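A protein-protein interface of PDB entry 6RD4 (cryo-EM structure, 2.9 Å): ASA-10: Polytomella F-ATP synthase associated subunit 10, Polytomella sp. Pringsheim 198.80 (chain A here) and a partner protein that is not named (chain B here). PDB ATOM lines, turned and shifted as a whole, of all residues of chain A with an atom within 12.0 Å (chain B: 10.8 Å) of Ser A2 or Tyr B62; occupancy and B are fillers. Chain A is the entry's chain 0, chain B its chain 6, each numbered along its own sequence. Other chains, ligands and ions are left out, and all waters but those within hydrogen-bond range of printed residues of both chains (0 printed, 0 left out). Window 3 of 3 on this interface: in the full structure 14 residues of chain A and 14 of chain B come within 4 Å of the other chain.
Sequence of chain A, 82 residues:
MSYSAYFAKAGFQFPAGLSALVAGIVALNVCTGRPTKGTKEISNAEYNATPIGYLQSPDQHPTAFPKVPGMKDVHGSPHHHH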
ATOM      1  N   SER A   2     -27.121  13.740  -3.000  1.00  0.00           N
ATOM      2  CA  SER A   2     -27.537  14.484  -4.163  1.00  0.00           C
ATOM      3  C   SER A   2     -28.845  15.124  -3.833  1.00  0.00           C
ATOM      4  O   SER A   2     -29.878  14.508  -3.994  1.00  0.00           O
ATOM      5  CB  SER A   2     -27.648  13.577  -5.380  1.00  0.00           C
ATOM      6  OG  SER A   2     -26.367  13.263  -5.894  1.00  0.00           O
ATOM      7  N   TYR A   3     -28.763  16.326  -3.262  1.00  0.00           N
ATOM      8  CA  TYR A   3     -29.855  17.231  -2.903  1.00  0.00           C
ATOM      9  C   TYR A   3     -30.748  16.722  -1.787  1.00  0.00           C
ATOM     10  O   TYR A   3     -31.611  17.461  -1.339  1.00  0.00           O
ATOM     11  CB  TYR A   3     -30.743  17.573  -4.097  1.00  0.00           C
ATOM     12  CG  TYR A   3     -30.129  18.488  -5.097  1.00  0.00           C
ATOM     13  CD1 TYR A   3     -29.358  19.538  -4.701  1.00  0.00           C
ATOM     14  CD2 TYR A   3     -30.325  18.290  -6.443  1.00  0.00           C
ATOM     15  CE1 TYR A   3     -28.786  20.346  -5.611  1.00  0.00           C
ATOM     16  CE2 TYR A   3     -29.763  19.103  -7.349  1.00  0.00           C
ATOM     17  CZ  TYR A   3     -28.991  20.125  -6.924  1.00  0.00           C
ATOM     18  OH  TYR A   3     -28.397  20.964  -7.813  1.00  0.00           O
ATOM     19  N   SER A   4     -30.565  15.494  -1.310  1.00  0.00           N
ATOM     20  CA  SER A   4     -31.370  15.027  -0.192  1.00  0.00           C
ATOM     21  C   SER A   4     -30.951  15.690   1.098  1.00  0.00           C
ATOM     22  O   SER A   4     -31.781  15.928   1.968  1.00  0.00           O
ATOM     23  CB  SER A   4     -31.262  13.520  -0.033  1.00  0.00           C
ATOM     24  OG  SER A   4     -31.942  12.842  -1.057  1.00  0.00           O
ATOM     25  N   ALA A   5     -29.678  15.996   1.235  1.00  0.00           N
ATOM     26  CA  ALA A   5     -29.154  16.636   2.420  1.00  0.00           C
ATOM     27  C   ALA A   5     -29.311  18.141   2.404  1.00  0.00           C
ATOM     28  O   ALA A   5     -28.979  18.786   3.394  1.00  0.00           O
ATOM     29  CB  ALA A   5     -27.686  16.287   2.563  1.00  0.00           C
ATOM     30  N   TYR A   6     -29.756  18.716   1.300  1.00  0.00           N
ATOM     31  CA  TYR A   6     -30.065  20.132   1.278  1.00  0.00           C
ATOM     32  C   TYR A   6     -31.443  20.394   1.844  1.00  0.00           C
ATOM     33  O   TYR A   6     -31.687  21.448   2.433  1.00  0.00           O
ATOM     34  CB  TYR A   6     -29.960  20.649  -0.150  1.00  0.00           C
ATOM     35  CG  TYR A   6     -30.508  22.016  -0.357  1.00  0.00           C
ATOM     36  CD1 TYR A   6     -29.916  23.102   0.222  1.00  0.00           C
ATOM     37  CD2 TYR A   6     -31.618  22.216  -1.125  1.00  0.00           C
ATOM     38  CE1 TYR A   6     -30.421  24.350   0.040  1.00  0.00           C
ATOM     39  CE2 TYR A   6     -32.124  23.453  -1.317  1.00  0.00           C
ATOM     40  CZ  TYR A   6     -31.527  24.518  -0.733  1.00  0.00           C
ATOM     41  OH  TYR A   6     -32.036  25.772  -0.916  1.00  0.00           O
ATOM     42  N   PHE A   7     -32.346  19.443   1.684  1.00  0.00           N
ATOM     43  CA  PHE A   7     -33.702  19.569   2.167  1.00  0.00           C
ATOM     44  C   PHE A   7     -33.870  19.095   3.589  1.00  0.00           C
ATOM     45  O   PHE A   7     -34.919  19.346   4.183  1.00  0.00           O
ATOM     46  CB  PHE A   7     -34.639  18.804   1.256  1.00  0.00           C
ATOM     47  CG  PHE A   7     -34.762  19.411  -0.071  1.00  0.00           C
ATOM     48  CD1 PHE A   7     -35.114  20.732  -0.194  1.00  0.00           C
ATOM     49  CD2 PHE A   7     -34.501  18.688  -1.190  1.00  0.00           C
ATOM     50  CE1 PHE A   7     -35.206  21.296  -1.406  1.00  0.00           C
ATOM     51  CE2 PHE A   7     -34.592  19.258  -2.400  1.00  0.00           C
ATOM     52  CZ  PHE A   7     -34.944  20.558  -2.502  1.00  0.00           C
ATOM     53  N   ALA A   8     -32.879  18.424   4.147  1.00  0.00           N
ATOM     54  CA  ALA A   8     -32.918  18.118   5.561  1.00  0.00           C
ATOM     55  C   ALA A   8     -32.410  19.262   6.414  1.00  0.00           C
ATOM     56  O   ALA A   8     -32.622  19.244   7.625  1.00  0.00           O
ATOM     57  CB  ALA A   8     -32.107  16.860   5.834  1.00  0.00           C
ATOM     58  N   LYS A   9     -31.759  20.254   5.816  1.00  0.00           N
ATOM     59  CA  LYS A   9     -31.162  21.343   6.577  1.00  0.00           C
ATOM     60  C   LYS A   9     -32.212  22.299   7.106  1.00  0.00           C
ATOM     61  O   LYS A   9     -32.224  22.621   8.295  1.00  0.00           O
ATOM     62  CB  LYS A   9     -30.159  22.101   5.721  1.00  0.00           C
ATOM     63  CG  LYS A   9     -28.904  21.332   5.482  1.00  0.00           C
ATOM     64  CD  LYS A   9     -28.007  22.065   4.532  1.00  0.00           C
ATOM     65  CE  LYS A   9     -26.813  21.223   4.193  1.00  0.00           C
ATOM     66  NZ  LYS A   9     -25.759  22.055   3.588  1.00  0.00           N
ATOM     67  N   GLU B  28     -20.488  33.435 -10.148  1.00  0.00           N
ATOM     68  CA  GLU B  28     -20.326  32.035 -10.509  1.00  0.00           C
ATOM     69  C   GLU B  28     -20.582  31.830 -11.995  1.00  0.00           C
ATOM     70  O   GLU B  28     -21.728  31.738 -12.426  1.00  0.00           O
ATOM     71  CB  GLU B  28     -21.268  31.166  -9.686  1.00  0.00           C
ATOM     72  CG  GLU B  28     -21.081  29.682  -9.891  1.00  0.00           C
ATOM     73  CD  GLU B  28     -22.067  28.861  -9.099  1.00  0.00           C
ATOM     74  OE1 GLU B  28     -23.053  29.433  -8.604  1.00  0.00           O
ATOM     75  OE2 GLU B  28     -21.854  27.645  -8.971  1.00  0.00           O
ATOM     76  N   LYS B  55     -13.508  17.079 -14.321  1.00  0.00           N
ATOM     77  CA  LYS B  55     -14.839  16.522 -14.148  1.00  0.00           C
ATOM     78  C   LYS B  55     -15.432  16.939 -12.819  1.00  0.00           C
ATOM     79  O   LYS B  55     -16.606  17.304 -12.744  1.00  0.00           O
ATOM     80  CB  LYS B  55     -14.776  15.005 -14.230  1.00  0.00           C
ATOM     81  CG  LYS B  55     -16.062  14.285 -14.016  1.00  0.00           C
ATOM     82  CD  LYS B  55     -16.855  14.231 -15.276  1.00  0.00           C
ATOM     83  CE  LYS B  55     -17.970  13.235 -15.166  1.00  0.00           C
ATOM     84  NZ  LYS B  55     -18.837  13.272 -16.367  1.00  0.00           N
ATOM     85  N   ALA B  56     -14.631  16.903 -11.763  1.00  0.00           N
ATOM     86  CA  ALA B  56     -15.103  17.201 -10.425  1.00  0.00           C
ATOM     87  C   ALA B  56     -15.089  18.681 -10.106  1.00  0.00           C
ATOM     88  O   ALA B  56     -15.708  19.086  -9.130  1.00  0.00           O
ATOM     89  CB  ALA B  56     -14.258  16.455  -9.407  1.00  0.00           C
ATOM     90  N   GLN B  57     -14.382  19.492 -10.876  1.00  0.00           N
ATOM     91  CA  GLN B  57     -14.475  20.930 -10.700  1.00  0.00           C
ATOM     92  C   GLN B  57     -15.739  21.497 -11.306  1.00  0.00           C
ATOM     93  O   GLN B  57     -16.097  22.638 -11.010  1.00  0.00           O
ATOM     94  CB  GLN B  57     -13.282  21.621 -11.334  1.00  0.00           C
ATOM     95  CG  GLN B  57     -12.176  21.947 -10.386  1.00  0.00           C
ATOM     96  CD  GLN B  57     -10.938  22.435 -11.101  1.00  0.00           C
ATOM     97  OE1 GLN B  57     -10.819  22.301 -12.315  1.00  0.00           O
ATOM     98  NE2 GLN B  57     -10.003  22.998 -10.350  1.00  0.00           N
ATOM     99  N   ALA B  58     -16.403  20.738 -12.167  1.00  0.00           N
ATOM    100  CA  ALA B  58     -17.616  21.171 -12.834  1.00  0.00           C
ATOM    101  C   ALA B  58     -18.805  20.307 -12.476  1.00  0.00           C
ATOM    102  O   ALA B  58     -19.846  20.414 -13.121  1.00  0.00           O
ATOM    103  CB  ALA B  58     -17.424  21.158 -14.339  1.00  0.00           C
ATOM    104  N   ALA B  59     -18.663  19.433 -11.497  1.00  0.00           N
ATOM    105  CA  ALA B  59     -19.799  18.742 -10.947  1.00  0.00           C
ATOM    106  C   ALA B  59     -20.646  19.734 -10.165  1.00  0.00           C
ATOM    107  O   ALA B  59     -20.121  20.710  -9.637  1.00  0.00           O
ATOM    108  CB  ALA B  59     -19.335  17.616 -10.040  1.00  0.00           C
ATOM    109  N   PRO B  60     -21.959  19.537 -10.103  1.00  0.00           N
ATOM    110  CA  PRO B  60     -22.789  20.449  -9.325  1.00  0.00           C
ATOM    111  C   PRO B  60     -22.621  20.203  -7.840  1.00  0.00           C
ATOM    112  O   PRO B  60     -22.235  19.123  -7.401  1.00  0.00           O
ATOM    113  CB  PRO B  60     -24.198  20.112  -9.788  1.00  0.00           C
ATOM    114  CG  PRO B  60     -24.109  18.750 -10.208  1.00  0.00           C
ATOM    115  CD  PRO B  60     -22.791  18.568 -10.826  1.00  0.00           C
ATOM    116  N   ILE B  61     -22.907  21.232  -7.058  1.00  0.00           N
ATOM    117  CA  ILE B  61     -22.802  21.101  -5.613  1.00  0.00           C
ATOM    118  C   ILE B  61     -24.016  20.343  -5.106  1.00  0.00           C
ATOM    119  O   ILE B  61     -25.155  20.640  -5.468  1.00  0.00           O
ATOM    120  CB  ILE B  61     -22.637  22.471  -4.934  1.00  0.00           C
ATOM    121  CG1 ILE B  61     -22.535  22.316  -3.429  1.00  0.00           C
ATOM    122  CG2 ILE B  61     -23.744  23.442  -5.256  1.00  0.00           C
ATOM    123  CD1 ILE B  61     -21.287  21.662  -2.998  1.00  0.00           C
ATOM    124  N   TYR B  62     -23.769  19.291  -4.363  1.00  0.00           N
ATOM    125  CA  TYR B  62     -24.807  18.640  -3.588  1.00  0.00           C
ATOM    126  C   TYR B  62     -24.377  18.810  -2.155  1.00  0.00           C
ATOM    127  O   TYR B  62     -23.424  18.132  -1.728  1.00  0.00           O
ATOM    128  CB  TYR B  62     -24.923  17.169  -3.946  1.00  0.00           C
ATOM    129  CG  TYR B  62     -25.208  16.915  -5.390  1.00  0.00           C
ATOM    130  CD1 TYR B  62     -26.153  17.639  -6.063  1.00  0.00           C
ATOM    131  CD2 TYR B  62     -24.528  15.940  -6.080  1.00  0.00           C
ATOM    132  CE1 TYR B  62     -26.412  17.402  -7.370  1.00  0.00           C
ATOM    133  CE2 TYR B  62     -24.786  15.705  -7.389  1.00  0.00           C
ATOM    134  CZ  TYR B  62     -25.732  16.439  -8.024  1.00  0.00           C
ATOM    135  OH  TYR B  62     -25.993  16.200  -9.336  1.00  0.00           O
ATOM    136  N   PRO B  63     -25.009  19.702  -1.395  1.00  0.00           N
ATOM    137  CA  PRO B  63     -24.486  20.079  -0.085  1.00  0.00           C
ATOM    138  C   PRO B  63     -24.491  18.930   0.900  1.00  0.00           C
ATOM    139  O   PRO B  63     -25.336  18.039   0.839  1.00  0.00           O
ATOM    140  CB  PRO B  63     -25.433  21.193   0.347  1.00  0.00           C
ATOM    141  CG  PRO B  63     -25.911  21.743  -0.894  1.00  0.00           C
ATOM    142  CD  PRO B  63     -26.086  20.601  -1.801  1.00  0.00           C
ATOM    143  N   ALA B  64     -23.479  18.915   1.752  1.00  0.00           N
ATOM    144  CA  ALA B  64     -23.228  17.755   2.575  1.00  0.00           C
ATOM    145  C   ALA B  64     -24.133  17.761   3.793  1.00  0.00           C
ATOM    146  O   ALA B  64     -24.577  18.808   4.263  1.00  0.00           O
ATOM    147  CB  ALA B  64     -21.766  17.707   3.000  1.00  0.00           C
ATOM    148  N   ALA B  65     -24.383  16.567   4.310  1.00  0.00           N
ATOM    149  CA  ALA B  65     -25.328  16.356   5.397  1.00  0.00           C
ATOM    150  C   ALA B  65     -24.766  16.948   6.673  1.00  0.00           C
ATOM    151  O   ALA B  65     -23.890  16.361   7.304  1.00  0.00           O
ATOM    152  CB  ALA B  65     -25.611  14.869   5.556  1.00  0.00           C
ATOM    153  N   ALA B  66     -25.275  18.109   7.064  1.00  0.00           N
ATOM    154  CA  ALA B  66     -24.772  18.779   8.252  1.00  0.00           C
ATOM    155  C   ALA B  66     -25.226  18.060   9.517  1.00  0.00           C
ATOM    156  O   ALA B  66     -25.978  17.081   9.477  1.00  0.00           O
ATOM    157  CB  ALA B  66     -25.232  20.235   8.281  1.00  0.00           C
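Among the printed residues, merely in contact across the chains: Ser A2 with Tyr B62 (3.3 Å), Lys A9 with Ala B64 (3.3 Å), Lys A9 with Pro B63 (3.4 Å), Ala A5 with Pro B63 (3.4 Å), Tyr A3 with Ile B61 (3.6 Å), Ala A5 with Ala B65 (3.7 Å) and Tyr A3 with Tyr B62 (3.8 Å).
Of chain B, only Tyr B62 (3.3 Å) comes within 4 Å of Ser A2.
Printed residues of chain B within 4 Å of Tyr A3: Ile B61 and Tyr B62.
Of the printed residues of chain B, Ala A5 touches Pro B63 (3.4 Å) and Ala B65 (3.7 Å).
Of the printed residues of chain B, Lys A9 touches Pro B63 and Ala B64.
Ala B56 touches none of the printed residues of chain A.
Gln B57 touches none of the printed residues of chain A.
No residue of chain A comes within 4 Å of Pro B60.
Ile B61 touches just one residue of chain A: Tyr A3 (3.6 Å).
Tyr B62 touches just these residues of chain A: Ser A2 and Tyr A3.
Pro B63 touches just these residues of chain A: Ala A5 and Lys A9.
Printed residues of chain A within 4 Å of Ala B65: Ala A5 (3.7 Å).
Of the 13 printed residues of chain B, 5 touch a printed residue of chain A.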
